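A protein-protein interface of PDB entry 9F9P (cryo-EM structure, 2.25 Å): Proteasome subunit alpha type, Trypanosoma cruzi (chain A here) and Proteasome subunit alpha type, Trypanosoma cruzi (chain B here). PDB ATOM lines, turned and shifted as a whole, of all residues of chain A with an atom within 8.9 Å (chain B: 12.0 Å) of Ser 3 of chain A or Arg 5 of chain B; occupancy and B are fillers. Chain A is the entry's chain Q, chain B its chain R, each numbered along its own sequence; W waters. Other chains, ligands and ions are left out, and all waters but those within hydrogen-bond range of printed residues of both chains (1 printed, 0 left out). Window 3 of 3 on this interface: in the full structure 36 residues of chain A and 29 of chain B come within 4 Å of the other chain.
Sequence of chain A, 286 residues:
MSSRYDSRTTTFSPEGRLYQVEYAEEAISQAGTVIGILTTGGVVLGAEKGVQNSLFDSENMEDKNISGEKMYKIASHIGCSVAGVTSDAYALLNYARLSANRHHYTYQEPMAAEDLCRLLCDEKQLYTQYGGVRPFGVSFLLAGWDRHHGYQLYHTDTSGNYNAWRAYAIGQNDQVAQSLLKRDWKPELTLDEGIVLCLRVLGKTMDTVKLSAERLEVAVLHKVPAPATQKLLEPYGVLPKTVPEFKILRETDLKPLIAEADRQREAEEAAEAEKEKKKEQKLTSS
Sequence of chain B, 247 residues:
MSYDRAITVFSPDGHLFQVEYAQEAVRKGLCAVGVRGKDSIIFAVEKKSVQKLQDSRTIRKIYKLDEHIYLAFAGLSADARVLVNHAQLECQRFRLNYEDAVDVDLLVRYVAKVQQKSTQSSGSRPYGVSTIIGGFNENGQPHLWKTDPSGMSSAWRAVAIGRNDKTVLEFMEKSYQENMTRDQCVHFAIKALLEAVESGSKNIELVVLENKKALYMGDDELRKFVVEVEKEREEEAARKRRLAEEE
The side-chain carboxylate of Asp 6 of chain A sits at hydrogen-bond distance from the backbone NH of Arg 8 of chain A (2.9 Å).
The backbone NH of Gly 123 of chain B sits at hydrogen-bond distance from the backbone carbonyl oxygen of Arg 5 of chain B (2.7 Å).
Of the 12 printed residues of chain A, 7 touch a printed residue of chain B.
Printed residues of chain A that touch a printed residue of chain B: Ser 3, Asp 6, Arg 8, Thr 10, Thr 11, Gly 131 and Gly 132.
Printed residues of chain B that touch a printed residue of chain A: Tyr 3, Arg 5, Ala 6, Ile 7, Gln 18, Gly 123 and Arg 125.
Hydrophobic or aromatic side chains of chain B within 4 Å of the printed part of chain A: Tyr 3 and Ile 7.
Among the printed residues, Asp or Glu carboxylates within 4 Å of a Lys or Arg side-chain nitrogen of the other chain: Asp 6 of chain A with Arg 5 of chain B (2.7 Å).
The side-chain carboxylate of Asp 6 of chain A is in salt-bridge range of the guanidinium group of Arg 5 of chain B (2.7 Å).
OD2 of Asp 6 of chain A sits at hydrogen-bond distance from OH of Tyr 3 of chain B, at 2.6 Å.
No residue of chain B comes within 4 Å of Ser 2 of chain A.
Ala 6 of chain B touches just one residue of chain A: Arg 8 (3.7 Å).
Printed residues of chain A within 4 Å of Ile 7 of chain B: Thr 11 (3.9 Å).
Printed residues of chain B within 4 Å of Thr 10 of chain A: Arg 125 (3.3 Å).
Of the printed residues of chain B, Gly 132 of chain A touches Tyr 3 (3.6 Å).
Ser 7 of chain A touches none of the printed residues of chain B.
Ser 124 of chain B touches none of the printed residues of chain A.
The nearest residue of chain B that does not touch Ser 3 of chain A is Tyr 3 of chain B (7.5 Å).
The nearest printed residue of chain B that does not touch Gly 132 of chain A is Gly 123 of chain B (5.2 Å).
Ser 3 of chain A touches Arg 5 of chain B.
Arg 8 of chain A touches Arg 5 of chain B.
Arg 8 of chain A touches Ala 6 of chain B (NH2 to O, 3.7 Å).
CB of Arg 125 of chain B touches O of Thr 10 of chain A, at 3.3 Å.
Thr 11 of chain A touches Ile 7 of chain B.
Gln 18 of chain B touches Thr 11 of chain A.
Gly 131 of chain A touches Tyr 3 of chain B (C to CB, 3.8 Å).
Gly 123 of chain B touches Gly 131 of chain A (O to N, 3.6 Å).
Gly 132 of chain A touches Tyr 3 of chain B.
Water W1 lies within hydrogen-bond range of OG1 of Thr 10 of chain A (2.7 Å) and OH of Tyr 3 of chain B (3.0 Å).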
ATOM      1  N   SER A   2       1.744 -21.764  37.769  1.00  0.00           N
ATOM      2  CA  SER A   2       1.897 -22.981  36.929  1.00  0.00           C
ATOM      3  C   SER A   2       0.949 -22.870  35.736  1.00  0.00           C
ATOM      4  O   SER A   2       1.326 -23.349  34.664  1.00  0.00           O
ATOM      5  CB  SER A   2       1.710 -24.321  37.661  1.00  0.00           C
ATOM      6  OG  SER A   2       2.841 -25.197  37.529  1.00  0.00           O
ATOM      7  N   SER A   3      -0.219 -22.210  35.876  1.00  0.00           N
ATOM      8  CA  SER A   3      -1.135 -22.081  34.744  1.00  0.00           C
ATOM      9  C   SER A   3      -0.587 -21.182  33.633  1.00  0.00           C
ATOM     10  O   SER A   3      -1.003 -21.325  32.499  1.00  0.00           O
ATOM     11  CB  SER A   3      -2.527 -21.629  35.132  1.00  0.00           C
ATOM     12  OG  SER A   3      -2.665 -20.219  35.000  1.00  0.00           O
ATOM     13  N   ARG A   4       0.370 -20.302  33.901  1.00  0.00           N
ATOM     14  CA  ARG A   4       0.915 -19.483  32.831  1.00  0.00           C
ATOM     15  C   ARG A   4       1.865 -20.256  31.913  1.00  0.00           C
ATOM     16  O   ARG A   4       2.253 -19.727  30.879  1.00  0.00           O
ATOM     17  CB  ARG A   4       1.614 -18.233  33.377  1.00  0.00           C
ATOM     18  CG  ARG A   4       2.627 -18.474  34.479  1.00  0.00           C
ATOM     19  CD  ARG A   4       2.893 -17.225  35.311  1.00  0.00           C
ATOM     20  NE  ARG A   4       3.751 -16.286  34.600  1.00  0.00           N
ATOM     21  CZ  ARG A   4       3.561 -14.970  34.532  1.00  0.00           C
ATOM     22  NH1 ARG A   4       4.366 -14.233  33.786  1.00  0.00           N
ATOM     23  NH2 ARG A   4       2.567 -14.397  35.197  1.00  0.00           N
ATOM     24  N   TYR A   5       2.271 -21.475  32.297  1.00  0.00           N
ATOM     25  CA  TYR A   5       3.126 -22.307  31.458  1.00  0.00           C
ATOM     26  C   TYR A   5       2.328 -23.437  30.794  1.00  0.00           C
ATOM     27  O   TYR A   5       2.935 -24.334  30.225  1.00  0.00           O
ATOM     28  CB  TYR A   5       4.309 -22.874  32.268  1.00  0.00           C
ATOM     29  CG  TYR A   5       5.080 -21.841  33.065  1.00  0.00           C
ATOM     30  CD1 TYR A   5       5.769 -20.814  32.433  1.00  0.00           C
ATOM     31  CD2 TYR A   5       5.021 -21.812  34.457  1.00  0.00           C
ATOM     32  CE1 TYR A   5       6.426 -19.825  33.158  1.00  0.00           C
ATOM     33  CE2 TYR A   5       5.648 -20.816  35.195  1.00  0.00           C
ATOM     34  CZ  TYR A   5       6.351 -19.816  34.545  1.00  0.00           C
ATOM     35  OH  TYR A   5       6.989 -18.843  35.289  1.00  0.00           O
ATOM     36  N   ASP A   6       0.984 -23.403  30.844  1.00  0.00           N
ATOM     37  CA  ASP A   6       0.154 -24.399  30.169  1.00  0.00           C
ATOM     38  C   ASP A   6       0.115 -24.058  28.681  1.00  0.00           C
ATOM     39  O   ASP A   6      -0.110 -22.912  28.337  1.00  0.00           O
ATOM     40  CB  ASP A   6      -1.241 -24.480  30.816  1.00  0.00           C
ATOM     41  CG  ASP A   6      -2.296 -25.422  30.226  1.00  0.00           C
ATOM     42  OD1 ASP A   6      -2.047 -26.015  29.173  1.00  0.00           O
ATOM     43  OD2 ASP A   6      -3.401 -25.533  30.830  1.00  0.00           O
ATOM     44  N   SER A   7       0.353 -25.050  27.814  1.00  0.00           N
ATOM     45  CA  SER A   7       0.405 -24.803  26.373  1.00  0.00           C
ATOM     46  C   SER A   7      -0.954 -24.954  25.671  1.00  0.00           C
ATOM     47  O   SER A   7      -1.049 -24.625  24.503  1.00  0.00           O
ATOM     48  CB  SER A   7       1.445 -25.695  25.738  1.00  0.00           C
ATOM     49  OG  SER A   7       1.035 -27.058  25.821  1.00  0.00           O
ATOM     50  N   ARG A   8      -1.994 -25.458  26.363  1.00  0.00           N
ATOM     51  CA  ARG A   8      -3.382 -25.449  25.894  1.00  0.00           C
ATOM     52  C   ARG A   8      -3.524 -26.305  24.626  1.00  0.00           C
ATOM     53  O   ARG A   8      -3.765 -25.804  23.533  1.00  0.00           O
ATOM     54  CB  ARG A   8      -3.874 -24.002  25.719  1.00  0.00           C
ATOM     55  CG  ARG A   8      -3.725 -23.129  26.965  1.00  0.00           C
ATOM     56  CD  ARG A   8      -4.671 -21.945  27.120  1.00  0.00           C
ATOM     57  NE  ARG A   8      -4.509 -21.251  28.407  1.00  0.00           N
ATOM     58  CZ  ARG A   8      -5.320 -21.368  29.472  1.00  0.00           C
ATOM     59  NH1 ARG A   8      -4.980 -20.812  30.629  1.00  0.00           N
ATOM     60  NH2 ARG A   8      -6.435 -22.082  29.401  1.00  0.00           N
ATOM     61  N   THR A   9      -3.339 -27.615  24.786  1.00  0.00           N
ATOM     62  CA  THR A   9      -3.287 -28.561  23.694  1.00  0.00           C
ATOM     63  C   THR A   9      -4.688 -28.850  23.132  1.00  0.00           C
ATOM     64  O   THR A   9      -4.813 -29.258  21.981  1.00  0.00           O
ATOM     65  CB  THR A   9      -2.618 -29.884  24.113  1.00  0.00           C
ATOM     66  OG1 THR A   9      -3.295 -30.582  25.171  1.00  0.00           O
ATOM     67  CG2 THR A   9      -1.175 -29.679  24.511  1.00  0.00           C
ATOM     68  N   THR A  10      -5.727 -28.734  23.962  1.00  0.00           N
ATOM     69  CA  THR A  10      -7.080 -29.074  23.530  1.00  0.00           C
ATOM     70  C   THR A  10      -7.949 -27.833  23.283  1.00  0.00           C
ATOM     71  O   THR A  10      -9.146 -27.952  23.304  1.00  0.00           O
ATOM     72  CB  THR A  10      -7.743 -30.021  24.541  1.00  0.00           C
ATOM     73  OG1 THR A  10      -7.657 -29.490  25.862  1.00  0.00           O
ATOM     74  CG2 THR A  10      -7.098 -31.391  24.520  1.00  0.00           C
ATOM     75  N   THR A  11      -7.356 -26.678  22.997  1.00  0.00           N
ATOM     76  CA  THR A  11      -8.064 -25.413  22.837  1.00  0.00           C
ATOM     77  C   THR A  11      -8.162 -25.123  21.336  1.00  0.00           C
ATOM     78  O   THR A  11      -7.186 -25.309  20.624  1.00  0.00           O
ATOM     79  CB  THR A  11      -7.321 -24.354  23.674  1.00  0.00           C
ATOM     80  OG1 THR A  11      -7.518 -24.585  25.074  1.00  0.00           O
ATOM     81  CG2 THR A  11      -7.729 -22.922  23.428  1.00  0.00           C
ATOM     82  N   GLY A 131      -8.422 -33.330  28.516  1.00  0.00           N
ATOM     83  CA  GLY A 131      -7.342 -33.801  29.374  1.00  0.00           C
ATOM     84  C   GLY A 131      -5.969 -33.137  29.222  1.00  0.00           C
ATOM     85  O   GLY A 131      -5.018 -33.577  29.876  1.00  0.00           O
ATOM     86  N   GLY A 132      -5.814 -32.070  28.456  1.00  0.00           N
ATOM     87  CA  GLY A 132      -4.571 -31.304  28.602  1.00  0.00           C
ATOM     88  C   GLY A 132      -3.206 -31.911  28.200  1.00  0.00           C
ATOM     89  O   GLY A 132      -2.202 -31.279  28.483  1.00  0.00           O
ATOM     90  N   SER B   2      -6.244 -34.845  37.011  1.00  0.00           N
ATOM     91  CA  SER B   2      -7.402 -34.455  36.158  1.00  0.00           C
ATOM     92  C   SER B   2      -7.321 -32.963  35.837  1.00  0.00           C
ATOM     93  O   SER B   2      -7.431 -32.116  36.724  1.00  0.00           O
ATOM     94  CB  SER B   2      -8.730 -34.803  36.802  1.00  0.00           C
ATOM     95  OG  SER B   2      -9.812 -34.530  35.918  1.00  0.00           O
ATOM     96  N   TYR B   3      -7.104 -32.682  34.552  1.00  0.00           N
ATOM     97  CA  TYR B   3      -7.056 -31.341  34.005  1.00  0.00           C
ATOM     98  C   TYR B   3      -8.410 -30.664  34.181  1.00  0.00           C
ATOM     99  O   TYR B   3      -9.401 -31.212  33.725  1.00  0.00           O
ATOM    100  CB  TYR B   3      -6.733 -31.442  32.517  1.00  0.00           C
ATOM    101  CG  TYR B   3      -6.362 -30.155  31.827  1.00  0.00           C
ATOM    102  CD1 TYR B   3      -5.245 -29.425  32.175  1.00  0.00           C
ATOM    103  CD2 TYR B   3      -7.140 -29.663  30.806  1.00  0.00           C
ATOM    104  CE1 TYR B   3      -4.900 -28.262  31.501  1.00  0.00           C
ATOM    105  CE2 TYR B   3      -6.780 -28.542  30.084  1.00  0.00           C
ATOM    106  CZ  TYR B   3      -5.660 -27.833  30.432  1.00  0.00           C
ATOM    107  OH  TYR B   3      -5.403 -26.720  29.687  1.00  0.00           O
ATOM    108  N   ASP B   4      -8.438 -29.485  34.823  1.00  0.00           N
ATOM    109  CA  ASP B   4      -9.694 -28.815  35.114  1.00  0.00           C
ATOM    110  C   ASP B   4      -9.609 -27.318  34.813  1.00  0.00           C
ATOM    111  O   ASP B   4     -10.300 -26.529  35.436  1.00  0.00           O
ATOM    112  CB  ASP B   4     -10.167 -29.124  36.549  1.00  0.00           C
ATOM    113  CG  ASP B   4      -9.272 -28.650  37.695  1.00  0.00           C
ATOM    114  OD1 ASP B   4      -8.640 -27.575  37.568  1.00  0.00           O
ATOM    115  OD2 ASP B   4      -9.252 -29.336  38.745  1.00  0.00           O
ATOM    116  N   ARG B   5      -8.752 -26.933  33.878  1.00  0.00           N
ATOM    117  CA  ARG B   5      -8.636 -25.571  33.409  1.00  0.00           C
ATOM    118  C   ARG B   5      -9.943 -25.136  32.740  1.00  0.00           C
ATOM    119  O   ARG B   5     -10.576 -25.913  32.036  1.00  0.00           O
ATOM    120  CB  ARG B   5      -7.496 -25.533  32.382  1.00  0.00           C
ATOM    121  CG  ARG B   5      -7.211 -24.191  31.718  1.00  0.00           C
ATOM    122  CD  ARG B   5      -6.049 -23.426  32.359  1.00  0.00           C
ATOM    123  NE  ARG B   5      -5.821 -23.716  33.780  1.00  0.00           N
ATOM    124  CZ  ARG B   5      -4.800 -24.429  34.271  1.00  0.00           C
ATOM    125  NH1 ARG B   5      -4.711 -24.633  35.574  1.00  0.00           N
ATOM    126  NH2 ARG B   5      -3.877 -24.941  33.471  1.00  0.00           N
ATOM    127  N   ALA B   6     -10.284 -23.851  32.891  1.00  0.00           N
ATOM    128  CA  ALA B   6     -11.370 -23.213  32.164  1.00  0.00           C
ATOM    129  C   ALA B   6     -10.923 -22.864  30.751  1.00  0.00           C
ATOM    130  O   ALA B   6      -9.948 -22.132  30.603  1.00  0.00           O
ATOM    131  CB  ALA B   6     -11.777 -21.961  32.893  1.00  0.00           C
ATOM    132  N   ILE B   7     -11.648 -23.358  29.740  1.00  0.00           N
ATOM    133  CA  ILE B   7     -11.268 -23.212  28.342  1.00  0.00           C
ATOM    134  C   ILE B   7     -12.194 -22.209  27.661  1.00  0.00           C
ATOM    135  O   ILE B   7     -11.734 -21.309  26.969  1.00  0.00           O
ATOM    136  CB  ILE B   7     -11.239 -24.601  27.643  1.00  0.00           C
ATOM    137  CG1 ILE B   7     -10.016 -25.422  28.071  1.00  0.00           C
ATOM    138  CG2 ILE B   7     -11.248 -24.471  26.136  1.00  0.00           C
ATOM    139  CD1 ILE B   7     -10.112 -26.919  27.772  1.00  0.00           C
ATOM    140  N   THR B   8     -13.501 -22.352  27.880  1.00  0.00           N
ATOM    141  CA  THR B   8     -14.492 -21.468  27.271  1.00  0.00           C
ATOM    142  C   THR B   8     -14.867 -20.319  28.225  1.00  0.00           C
ATOM    143  O   THR B   8     -15.556 -20.537  29.211  1.00  0.00           O
ATOM    144  CB  THR B   8     -15.740 -22.295  26.886  1.00  0.00           C
ATOM    145  OG1 THR B   8     -15.476 -23.476  26.121  1.00  0.00           O
ATOM    146  CG2 THR B   8     -16.730 -21.485  26.094  1.00  0.00           C
ATOM    147  N   VAL B   9     -14.420 -19.093  27.952  1.00  0.00           N
ATOM    148  CA  VAL B   9     -14.680 -17.975  28.852  1.00  0.00           C
ATOM    149  C   VAL B   9     -15.196 -16.789  28.050  1.00  0.00           C
ATOM    150  O   VAL B   9     -14.929 -16.688  26.858  1.00  0.00           O
ATOM    151  CB  VAL B   9     -13.416 -17.577  29.654  1.00  0.00           C
ATOM    152  CG1 VAL B   9     -12.984 -18.684  30.598  1.00  0.00           C
ATOM    153  CG2 VAL B   9     -12.251 -17.182  28.759  1.00  0.00           C
ATOM    154  N   PHE B  10     -15.870 -15.857  28.726  1.00  0.00           N
ATOM    155  CA  PHE B  10     -16.280 -14.625  28.077  1.00  0.00           C
ATOM    156  C   PHE B  10     -15.065 -13.752  27.899  1.00  0.00           C
ATOM    157  O   PHE B  10     -14.171 -13.766  28.733  1.00  0.00           O
ATOM    158  CB  PHE B  10     -17.286 -13.785  28.873  1.00  0.00           C
ATOM    159  CG  PHE B  10     -18.672 -14.340  28.917  1.00  0.00           C
ATOM    160  CD1 PHE B  10     -19.543 -14.127  27.873  1.00  0.00           C
ATOM    161  CD2 PHE B  10     -19.075 -15.141  29.957  1.00  0.00           C
ATOM    162  CE1 PHE B  10     -20.811 -14.698  27.865  1.00  0.00           C
ATOM    163  CE2 PHE B  10     -20.357 -15.697  29.964  1.00  0.00           C
ATOM    164  CZ  PHE B  10     -21.208 -15.513  28.903  1.00  0.00           C
ATOM    165  N   GLN B  18     -14.201 -19.590  22.044  1.00  0.00           N
ATOM    166  CA  GLN B  18     -14.168 -20.999  21.731  1.00  0.00           C
ATOM    167  C   GLN B  18     -15.436 -21.445  20.995  1.00  0.00           C
ATOM    168  O   GLN B  18     -15.381 -22.418  20.236  1.00  0.00           O
ATOM    169  CB  GLN B  18     -13.985 -21.870  22.980  1.00  0.00           C
ATOM    170  CG  GLN B  18     -12.589 -21.851  23.600  1.00  0.00           C
ATOM    171  CD  GLN B  18     -11.534 -22.328  22.646  1.00  0.00           C
ATOM    172  OE1 GLN B  18     -11.427 -23.518  22.402  1.00  0.00           O
ATOM    173  NE2 GLN B  18     -10.734 -21.410  22.129  1.00  0.00           N
ATOM    174  N   LYS B 117     -23.433 -28.349  27.280  1.00  0.00           N
ATOM    175  CA  LYS B 117     -22.571 -28.642  28.406  1.00  0.00           C
ATOM    176  C   LYS B 117     -21.095 -28.570  28.054  1.00  0.00           C
ATOM    177  O   LYS B 117     -20.291 -28.291  28.931  1.00  0.00           O
ATOM    178  CB  LYS B 117     -22.834 -30.022  29.010  1.00  0.00           C
ATOM    179  CG  LYS B 117     -24.039 -30.037  29.930  1.00  0.00           C
ATOM    180  CD  LYS B 117     -24.258 -31.335  30.650  1.00  0.00           C
ATOM    181  CE  LYS B 117     -25.671 -31.393  31.198  1.00  0.00           C
ATOM    182  NZ  LYS B 117     -25.940 -32.682  31.886  1.00  0.00           N
ATOM    183  N   SER B 118     -20.745 -28.950  26.821  1.00  0.00           N
ATOM    184  CA  SER B 118     -19.368 -28.897  26.365  1.00  0.00           C
ATOM    185  C   SER B 118     -18.878 -27.458  26.295  1.00  0.00           C
ATOM    186  O   SER B 118     -17.678 -27.262  26.313  1.00  0.00           O
ATOM    187  CB  SER B 118     -19.183 -29.641  25.047  1.00  0.00           C
ATOM    188  OG  SER B 118     -19.746 -28.941  23.949  1.00  0.00           O
ATOM    189  N   THR B 119     -19.776 -26.458  26.323  1.00  0.00           N
ATOM    190  CA  THR B 119     -19.342 -25.066  26.267  1.00  0.00           C
ATOM    191  C   THR B 119     -19.176 -24.451  27.650  1.00  0.00           C
ATOM    192  O   THR B 119     -18.910 -23.262  27.729  1.00  0.00           O
ATOM    193  CB  THR B 119     -20.331 -24.146  25.528  1.00  0.00           C
ATOM    194  OG1 THR B 119     -21.553 -24.040  26.258  1.00  0.00           O
ATOM    195  CG2 THR B 119     -20.630 -24.643  24.131  1.00  0.00           C
ATOM    196  N   GLN B 120     -19.386 -25.232  28.711  1.00  0.00           N
ATOM    197  CA  GLN B 120     -19.362 -24.704  30.076  1.00  0.00           C
ATOM    198  C   GLN B 120     -18.617 -25.614  31.073  1.00  0.00           C
ATOM    199  O   GLN B 120     -18.530 -25.316  32.248  1.00  0.00           O
ATOM    200  CB  GLN B 120     -20.804 -24.507  30.545  1.00  0.00           C
ATOM    201  CG  GLN B 120     -20.954 -23.372  31.525  1.00  0.00           C
ATOM    202  CD  GLN B 120     -22.398 -23.069  31.892  1.00  0.00           C
ATOM    203  OE1 GLN B 120     -23.323 -23.815  31.560  1.00  0.00           O
ATOM    204  NE2 GLN B 120     -22.600 -21.946  32.560  1.00  0.00           N
ATOM    205  N   SER B 121     -18.098 -26.743  30.607  1.00  0.00           N
ATOM    206  CA  SER B 121     -17.433 -27.690  31.468  1.00  0.00           C
ATOM    207  C   SER B 121     -15.948 -27.368  31.463  1.00  0.00           C
ATOM    208  O   SER B 121     -15.363 -27.151  30.405  1.00  0.00           O
ATOM    209  CB  SER B 121     -17.684 -29.123  31.032  1.00  0.00           C
ATOM    210  OG  SER B 121     -16.928 -29.439  29.852  1.00  0.00           O
ATOM    211  N   SER B 122     -15.365 -27.343  32.654  1.00  0.00           N
ATOM    212  CA  SER B 122     -13.935 -27.136  32.785  1.00  0.00           C
ATOM    213  C   SER B 122     -13.206 -28.369  32.254  1.00  0.00           C
ATOM    214  O   SER B 122     -13.704 -29.493  32.387  1.00  0.00           O
ATOM    215  CB  SER B 122     -13.594 -26.875  34.223  1.00  0.00           C
ATOM    216  OG  SER B 122     -14.272 -25.711  34.687  1.00  0.00           O
ATOM    217  N   GLY B 123     -12.054 -28.141  31.613  1.00  0.00           N
ATOM    218  CA  GLY B 123     -11.211 -29.255  31.238  1.00  0.00           C
ATOM    219  C   GLY B 123     -11.471 -29.804  29.826  1.00  0.00           C
ATOM    220  O   GLY B 123     -10.776 -30.733  29.414  1.00  0.00           O
ATOM    221  N   SER B 124     -12.388 -29.194  29.063  1.00  0.00           N
ATOM    222  CA  SER B 124     -12.757 -29.718  27.760  1.00  0.00           C
ATOM    223  C   SER B 124     -13.200 -28.603  26.817  1.00  0.00           C
ATOM    224  O   SER B 124     -13.708 -27.592  27.278  1.00  0.00           O
ATOM    225  CB  SER B 124     -13.829 -30.778  27.958  1.00  0.00           C
ATOM    226  OG  SER B 124     -14.278 -31.320  26.719  1.00  0.00           O
ATOM    227  N   ARG B 125     -12.961 -28.770  25.503  1.00  0.00           N
ATOM    228  CA  ARG B 125     -13.394 -27.804  24.493  1.00  0.00           C
ATOM    229  C   ARG B 125     -14.757 -28.223  23.923  1.00  0.00           C
ATOM    230  O   ARG B 125     -15.145 -29.380  24.052  1.00  0.00           O
ATOM    231  CB  ARG B 125     -12.401 -27.693  23.327  1.00  0.00           C
ATOM    232  CG  ARG B 125     -12.277 -28.972  22.514  1.00  0.00           C
ATOM    233  CD  ARG B 125     -11.587 -28.778  21.180  1.00  0.00           C
ATOM    234  NE  ARG B 125     -11.270 -30.071  20.594  1.00  0.00           N
ATOM    235  CZ  ARG B 125     -12.110 -30.817  19.873  1.00  0.00           C
ATOM    236  NH1 ARG B 125     -13.330 -30.379  19.600  1.00  0.00           N
ATOM    237  NH2 ARG B 125     -11.724 -31.995  19.421  1.00  0.00           N
ATOM    238  N   PRO B 126     -15.505 -27.313  23.257  1.00  0.00           N
ATOM    239  CA  PRO B 126     -16.733 -27.667  22.537  1.00  0.00           C
ATOM    240  C   PRO B 126     -16.573 -28.666  21.383  1.00  0.00           C
ATOM    241  O   PRO B 126     -15.503 -28.744  20.782  1.00  0.00           O
ATOM    242  CB  PRO B 126     -17.236 -26.363  21.919  1.00  0.00           C
ATOM    243  CG  PRO B 126     -16.426 -25.249  22.553  1.00  0.00           C
ATOM    244  CD  PRO B 126     -15.182 -25.885  23.139  1.00  0.00           C
HETATM  245  O   HOH W   1      -6.390 -27.397  26.948  1.00  0.00           O
